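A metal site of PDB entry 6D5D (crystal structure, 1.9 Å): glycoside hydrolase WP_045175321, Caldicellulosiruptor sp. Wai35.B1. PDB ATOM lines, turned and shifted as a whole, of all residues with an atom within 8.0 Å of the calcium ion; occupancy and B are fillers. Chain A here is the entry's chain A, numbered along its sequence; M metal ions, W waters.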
ATOM      1  N   GLU A 124     -11.292  -9.050  13.050  1.00  0.00           N
ATOM      2  CA  GLU A 124     -11.024 -10.404  13.507  1.00  0.00           C
ATOM      3  C   GLU A 124      -9.862 -11.114  12.855  1.00  0.00           C
ATOM      4  O   GLU A 124      -9.242 -11.989  13.493  1.00  0.00           O
ATOM      5  CB  GLU A 124     -12.299 -11.280  13.365  1.00  0.00           C
ATOM      6  CG  GLU A 124     -13.400 -11.030  14.407  1.00  0.00           C
ATOM      7  CD  GLU A 124     -14.388  -9.860  14.061  1.00  0.00           C
ATOM      8  OE1 GLU A 124     -14.089  -9.044  13.140  1.00  0.00           O
ATOM      9  OE2 GLU A 124     -15.456  -9.720  14.763  1.00  0.00           O
ATOM     10  N   THR A 125      -9.523 -10.777  11.613  1.00  0.00           N
ATOM     11  CA  THR A 125      -8.407 -11.395  10.938  1.00  0.00           C
ATOM     12  C   THR A 125      -7.563 -10.329  10.264  1.00  0.00           C
ATOM     13  O   THR A 125      -8.098  -9.239   9.947  1.00  0.00           O
ATOM     14  CB  THR A 125      -8.882 -12.508   9.960  1.00  0.00           C
ATOM     15  OG1 THR A 125      -9.804 -11.965   8.999  1.00  0.00           O
ATOM     16  CG2 THR A 125      -9.656 -13.662  10.746  1.00  0.00           C
ATOM     17  N   PRO A 126      -6.266 -10.580  10.081  1.00  0.00           N
ATOM     18  CA  PRO A 126      -5.361  -9.653   9.387  1.00  0.00           C
ATOM     19  C   PRO A 126      -5.772  -9.291   7.959  1.00  0.00           C
ATOM     20  O   PRO A 126      -5.520  -8.148   7.501  1.00  0.00           O
ATOM     21  CB  PRO A 126      -4.049 -10.423   9.362  1.00  0.00           C
ATOM     22  CG  PRO A 126      -4.141 -11.412  10.470  1.00  0.00           C
ATOM     23  CD  PRO A 126      -5.551 -11.767  10.595  1.00  0.00           C
ATOM     24  N   GLY A 191      -5.056  -6.588  14.539  1.00  0.00           N
ATOM     25  CA  GLY A 191      -6.162  -7.209  15.290  1.00  0.00           C
ATOM     26  C   GLY A 191      -5.747  -8.479  16.008  1.00  0.00           C
ATOM     27  O   GLY A 191      -4.540  -8.803  16.063  1.00  0.00           O
ATOM     28  N   PRO A 192      -6.716  -9.191  16.549  1.00  0.00           N
ATOM     29  CA  PRO A 192      -6.436 -10.281  17.511  1.00  0.00           C
ATOM     30  C   PRO A 192      -5.846 -11.563  16.942  1.00  0.00           C
ATOM     31  O   PRO A 192      -5.272 -12.357  17.696  1.00  0.00           O
ATOM     32  CB  PRO A 192      -7.793 -10.560  18.142  1.00  0.00           C
ATOM     33  CG  PRO A 192      -8.792  -9.878  17.322  1.00  0.00           C
ATOM     34  CD  PRO A 192      -8.129  -8.769  16.599  1.00  0.00           C
ATOM     35  N   GLU A 193      -5.965 -11.753  15.628  1.00  0.00           N
ATOM     36  CA  GLU A 193      -5.413 -12.939  14.986  1.00  0.00           C
ATOM     37  C   GLU A 193      -4.079 -12.659  14.334  1.00  0.00           C
ATOM     38  O   GLU A 193      -3.521 -13.529  13.701  1.00  0.00           O
ATOM     39  CB  GLU A 193      -6.414 -13.538  13.956  1.00  0.00           C
ATOM     40  CG  GLU A 193      -7.415 -14.521  14.563  1.00  0.00           C
ATOM     41  CD  GLU A 193      -6.734 -15.866  14.951  1.00  0.00           C
ATOM     42  OE1 GLU A 193      -5.581 -16.199  14.483  1.00  0.00           O
ATOM     43  OE2 GLU A 193      -7.358 -16.621  15.689  1.00  0.00           O
ATOM     44  N   GLU A 194      -3.545 -11.463  14.443  1.00  0.00           N
ATOM     45  CA  GLU A 194      -2.203 -11.217  13.902  1.00  0.00           C
ATOM     46  C   GLU A 194      -1.169 -11.702  14.894  1.00  0.00           C
ATOM     47  O   GLU A 194      -0.730 -10.935  15.763  1.00  0.00           O
ATOM     48  CB  GLU A 194      -2.013  -9.738  13.563  1.00  0.00           C
ATOM     49  CG  GLU A 194      -0.738  -9.428  12.782  1.00  0.00           C
ATOM     50  CD  GLU A 194      -0.448  -7.978  12.621  1.00  0.00           C
ATOM     51  OE1 GLU A 194      -0.685  -7.257  13.607  1.00  0.00           O
ATOM     52  OE2 GLU A 194       0.015  -7.534  11.505  1.00  0.00           O
ATOM     53  N   SER A 195      -0.730 -12.947  14.768  1.00  0.00           N
ATOM     54  CA  SER A 195       0.344 -13.480  15.616  1.00  0.00           C
ATOM     55  C   SER A 195       1.668 -12.793  15.371  1.00  0.00           C
ATOM     56  O   SER A 195       1.892 -12.090  14.316  1.00  0.00           O
ATOM     57  CB  SER A 195       0.529 -14.992  15.411  1.00  0.00           C
ATOM     58  OG  SER A 195       1.103 -15.319  14.178  1.00  0.00           O
ATOM     59  N   VAL A 196       2.617 -13.088  16.267  1.00  0.00           N
ATOM     60  CA  VAL A 196       3.955 -12.603  16.113  1.00  0.00           C
ATOM     61  C   VAL A 196       4.536 -12.953  14.728  1.00  0.00           C
ATOM     62  O   VAL A 196       5.426 -12.271  14.219  1.00  0.00           O
ATOM     63  CB  VAL A 196       4.853 -13.131  17.267  1.00  0.00           C
ATOM     64  CG1 VAL A 196       5.006 -14.633  17.250  1.00  0.00           C
ATOM     65  CG2 VAL A 196       6.192 -12.456  17.162  1.00  0.00           C
ATOM     66  N   TRP A 197       4.013 -14.017  14.159  1.00  0.00           N
ATOM     67  CA  TRP A 197       4.485 -14.539  12.870  1.00  0.00           C
ATOM     68  C   TRP A 197       3.889 -13.831  11.627  1.00  0.00           C
ATOM     69  O   TRP A 197       4.365 -14.072  10.488  1.00  0.00           O
ATOM     70  CB  TRP A 197       4.189 -16.036  12.791  1.00  0.00           C
ATOM     71  CG  TRP A 197       4.717 -16.840  13.916  1.00  0.00           C
ATOM     72  CD1 TRP A 197       4.053 -17.245  15.062  1.00  0.00           C
ATOM     73  CD2 TRP A 197       6.081 -17.307  14.053  1.00  0.00           C
ATOM     74  NE1 TRP A 197       4.931 -17.917  15.893  1.00  0.00           N
ATOM     75  CE2 TRP A 197       6.173 -17.943  15.319  1.00  0.00           C
ATOM     76  CE3 TRP A 197       7.223 -17.159  13.290  1.00  0.00           C
ATOM     77  CZ2 TRP A 197       7.345 -18.512  15.772  1.00  0.00           C
ATOM     78  CZ3 TRP A 197       8.404 -17.748  13.743  1.00  0.00           C
ATOM     79  CH2 TRP A 197       8.452 -18.399  14.987  1.00  0.00           C
ATOM     80  N   GLU A 198       2.914 -12.951  11.830  1.00  0.00           N
ATOM     81  CA  GLU A 198       2.052 -12.482  10.764  1.00  0.00           C
ATOM     82  C   GLU A 198       2.059 -10.979  10.610  1.00  0.00           C
ATOM     83  O   GLU A 198       1.176 -10.391   9.932  1.00  0.00           O
ATOM     84  CB  GLU A 198       0.634 -12.961  11.050  1.00  0.00           C
ATOM     85  CG  GLU A 198       0.428 -14.432  10.894  1.00  0.00           C
ATOM     86  CD  GLU A 198      -0.950 -14.855  11.406  1.00  0.00           C
ATOM     87  OE1 GLU A 198      -1.956 -14.735  10.695  1.00  0.00           O
ATOM     88  OE2 GLU A 198      -1.046 -15.240  12.605  1.00  0.00           O
ATOM     89  N   ARG A 416      -5.474 -13.676  20.332  1.00  0.00           N
ATOM     90  CA  ARG A 416      -6.016 -15.052  20.261  1.00  0.00           C
ATOM     91  C   ARG A 416      -5.107 -16.055  19.579  1.00  0.00           C
ATOM     92  O   ARG A 416      -5.479 -17.243  19.464  1.00  0.00           O
ATOM     93  CB  ARG A 416      -7.351 -15.077  19.483  1.00  0.00           C
ATOM     94  CG  ARG A 416      -8.378 -14.032  19.885  1.00  0.00           C
ATOM     95  CD  ARG A 416      -9.168 -14.427  21.134  1.00  0.00           C
ATOM     96  NE  ARG A 416      -9.458 -13.247  21.957  1.00  0.00           N
ATOM     97  CZ  ARG A 416     -10.233 -12.223  21.606  1.00  0.00           C
ATOM     98  NH1 ARG A 416     -10.845 -12.198  20.411  1.00  0.00           N
ATOM     99  NH2 ARG A 416     -10.389 -11.219  22.456  1.00  0.00           N
ATOM    100  N   ASP A 417      -3.896 -15.635  19.178  1.00  0.00           N
ATOM    101  CA  ASP A 417      -2.976 -16.519  18.435  1.00  0.00           C
ATOM    102  C   ASP A 417      -1.554 -16.373  18.987  1.00  0.00           C
ATOM    103  O   ASP A 417      -0.598 -15.815  18.324  1.00  0.00           O
ATOM    104  CB  ASP A 417      -3.056 -16.287  16.913  1.00  0.00           C
ATOM    105  CG  ASP A 417      -2.222 -17.369  16.129  1.00  0.00           C
ATOM    106  OD1 ASP A 417      -1.737 -18.390  16.711  1.00  0.00           O
ATOM    107  OD2 ASP A 417      -1.996 -17.165  14.915  1.00  0.00           O
ATOM    108  N   PRO A 418      -1.355 -16.932  20.193  1.00  0.00           N
ATOM    109  CA  PRO A 418      -2.266 -17.727  21.012  1.00  0.00           C
ATOM    110  C   PRO A 418      -3.084 -16.798  21.958  1.00  0.00           C
ATOM    111  O   PRO A 418      -2.782 -15.577  22.043  1.00  0.00           O
ATOM    112  CB  PRO A 418      -1.286 -18.598  21.821  1.00  0.00           C
ATOM    113  CG  PRO A 418      -0.209 -17.579  22.186  1.00  0.00           C
ATOM    114  CD  PRO A 418      -0.012 -16.837  20.839  1.00  0.00           C
ATOM    115  N   ARG A 564       6.653 -22.041  11.770  1.00  0.00           N
ATOM    116  CA  ARG A 564       6.006 -20.843  11.231  1.00  0.00           C
ATOM    117  C   ARG A 564       7.035 -19.917  10.635  1.00  0.00           C
ATOM    118  O   ARG A 564       6.661 -19.136   9.804  1.00  0.00           O
ATOM    119  CB  ARG A 564       5.113 -20.130  12.287  1.00  0.00           C
ATOM    120  CG  ARG A 564       3.821 -20.926  12.602  1.00  0.00           C
ATOM    121  CD  ARG A 564       2.968 -20.338  13.710  1.00  0.00           C
ATOM    122  NE  ARG A 564       1.882 -19.471  13.190  1.00  0.00           N
ATOM    123  CZ  ARG A 564       0.918 -18.963  13.920  1.00  0.00           C
ATOM    124  NH1 ARG A 564       0.896 -19.134  15.267  1.00  0.00           N
ATOM    125  NH2 ARG A 564      -0.021 -18.211  13.328  1.00  0.00           N
ATOM    126  N   GLN A 568       4.454 -19.680   7.585  1.00  0.00           N
ATOM    127  CA  GLN A 568       3.399 -18.715   7.927  1.00  0.00           C
ATOM    128  C   GLN A 568       3.310 -17.680   6.836  1.00  0.00           C
ATOM    129  O   GLN A 568       4.239 -16.938   6.621  1.00  0.00           O
ATOM    130  CB  GLN A 568       3.618 -17.982   9.249  1.00  0.00           C
ATOM    131  CG  GLN A 568       2.486 -16.963   9.591  1.00  0.00           C
ATOM    132  CD  GLN A 568       1.159 -17.596   9.778  1.00  0.00           C
ATOM    133  OE1 GLN A 568       1.013 -18.402  10.670  1.00  0.00           O
ATOM    134  NE2 GLN A 568       0.150 -17.244   8.911  1.00  0.00           N
ATOM    135  N   GLU A 569       2.172 -17.625   6.173  1.00  0.00           N
ATOM    136  CA  GLU A 569       1.913 -16.526   5.229  1.00  0.00           C
ATOM    137  C   GLU A 569       1.653 -15.224   5.965  1.00  0.00           C
ATOM    138  O   GLU A 569       0.903 -15.228   6.920  1.00  0.00           O
ATOM    139  CB  GLU A 569       0.684 -16.825   4.396  1.00  0.00           C
ATOM    140  CG  GLU A 569       0.476 -15.740   3.309  1.00  0.00           C
ATOM    141  CD  GLU A 569      -0.438 -16.221   2.190  1.00  0.00           C
ATOM    142  OE1 GLU A 569      -0.307 -17.391   1.768  1.00  0.00           O
ATOM    143  OE2 GLU A 569      -1.267 -15.409   1.749  1.00  0.00           O
HETATM  144 CA    CA M   1      -3.235 -15.833  13.267  1.00  0.00          CA
HETATM  145  O   HOH W   1      -4.337 -15.817  11.063  1.00  0.00           O
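The calcium ion is bound by the backbone carbonyl oxygen (O) of Glu 193 (2.4 Å), the side-chain carboxylate (OE2) of Glu 198 (2.4 Å), the side-chain carboxylate (OD2) of Asp 417 (2.5 Å), water W1 (2.5 Å) and the side-chain carboxylate (OE1) of Glu 193 (2.7 Å).
The calcium ion has five donor atoms within binding distance.
Slightly farther from the calcium ion lies the side-chain carboxylate (OE1) of Glu 198 (3.1 Å).
The side-chain carboxylate (OE2) of Glu 198 sits close to the guanidinium group (NH2) of Arg 564 (3.2 Å).
The guanidinium group (NH2) of Arg 564 sits at hydrogen-bond distance from the side-chain amide oxygen (OE1) of Gln 568, 2.9 Å away.
The guanidinium group of Arg 564 is in hydrogen-bond range of the side-chain hydroxyl of Ser 195 (3.2 Å).
The side-chain hydroxyl of Ser 195 sits close to the side-chain carboxylate of Glu 198 (2.7 Å).
The guanidinium group (NH1) of Arg 564 is in salt-bridge range of the side-chain carboxylate (OD1) of Asp 417, 3.1 Å away.
Merely in contact with the calcium ion: Arg 564 (3.999 Å).
Four residues have an atom within 4 Å of the calcium ion: Glu 193, Glu 198, Asp 417 and Arg 564.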
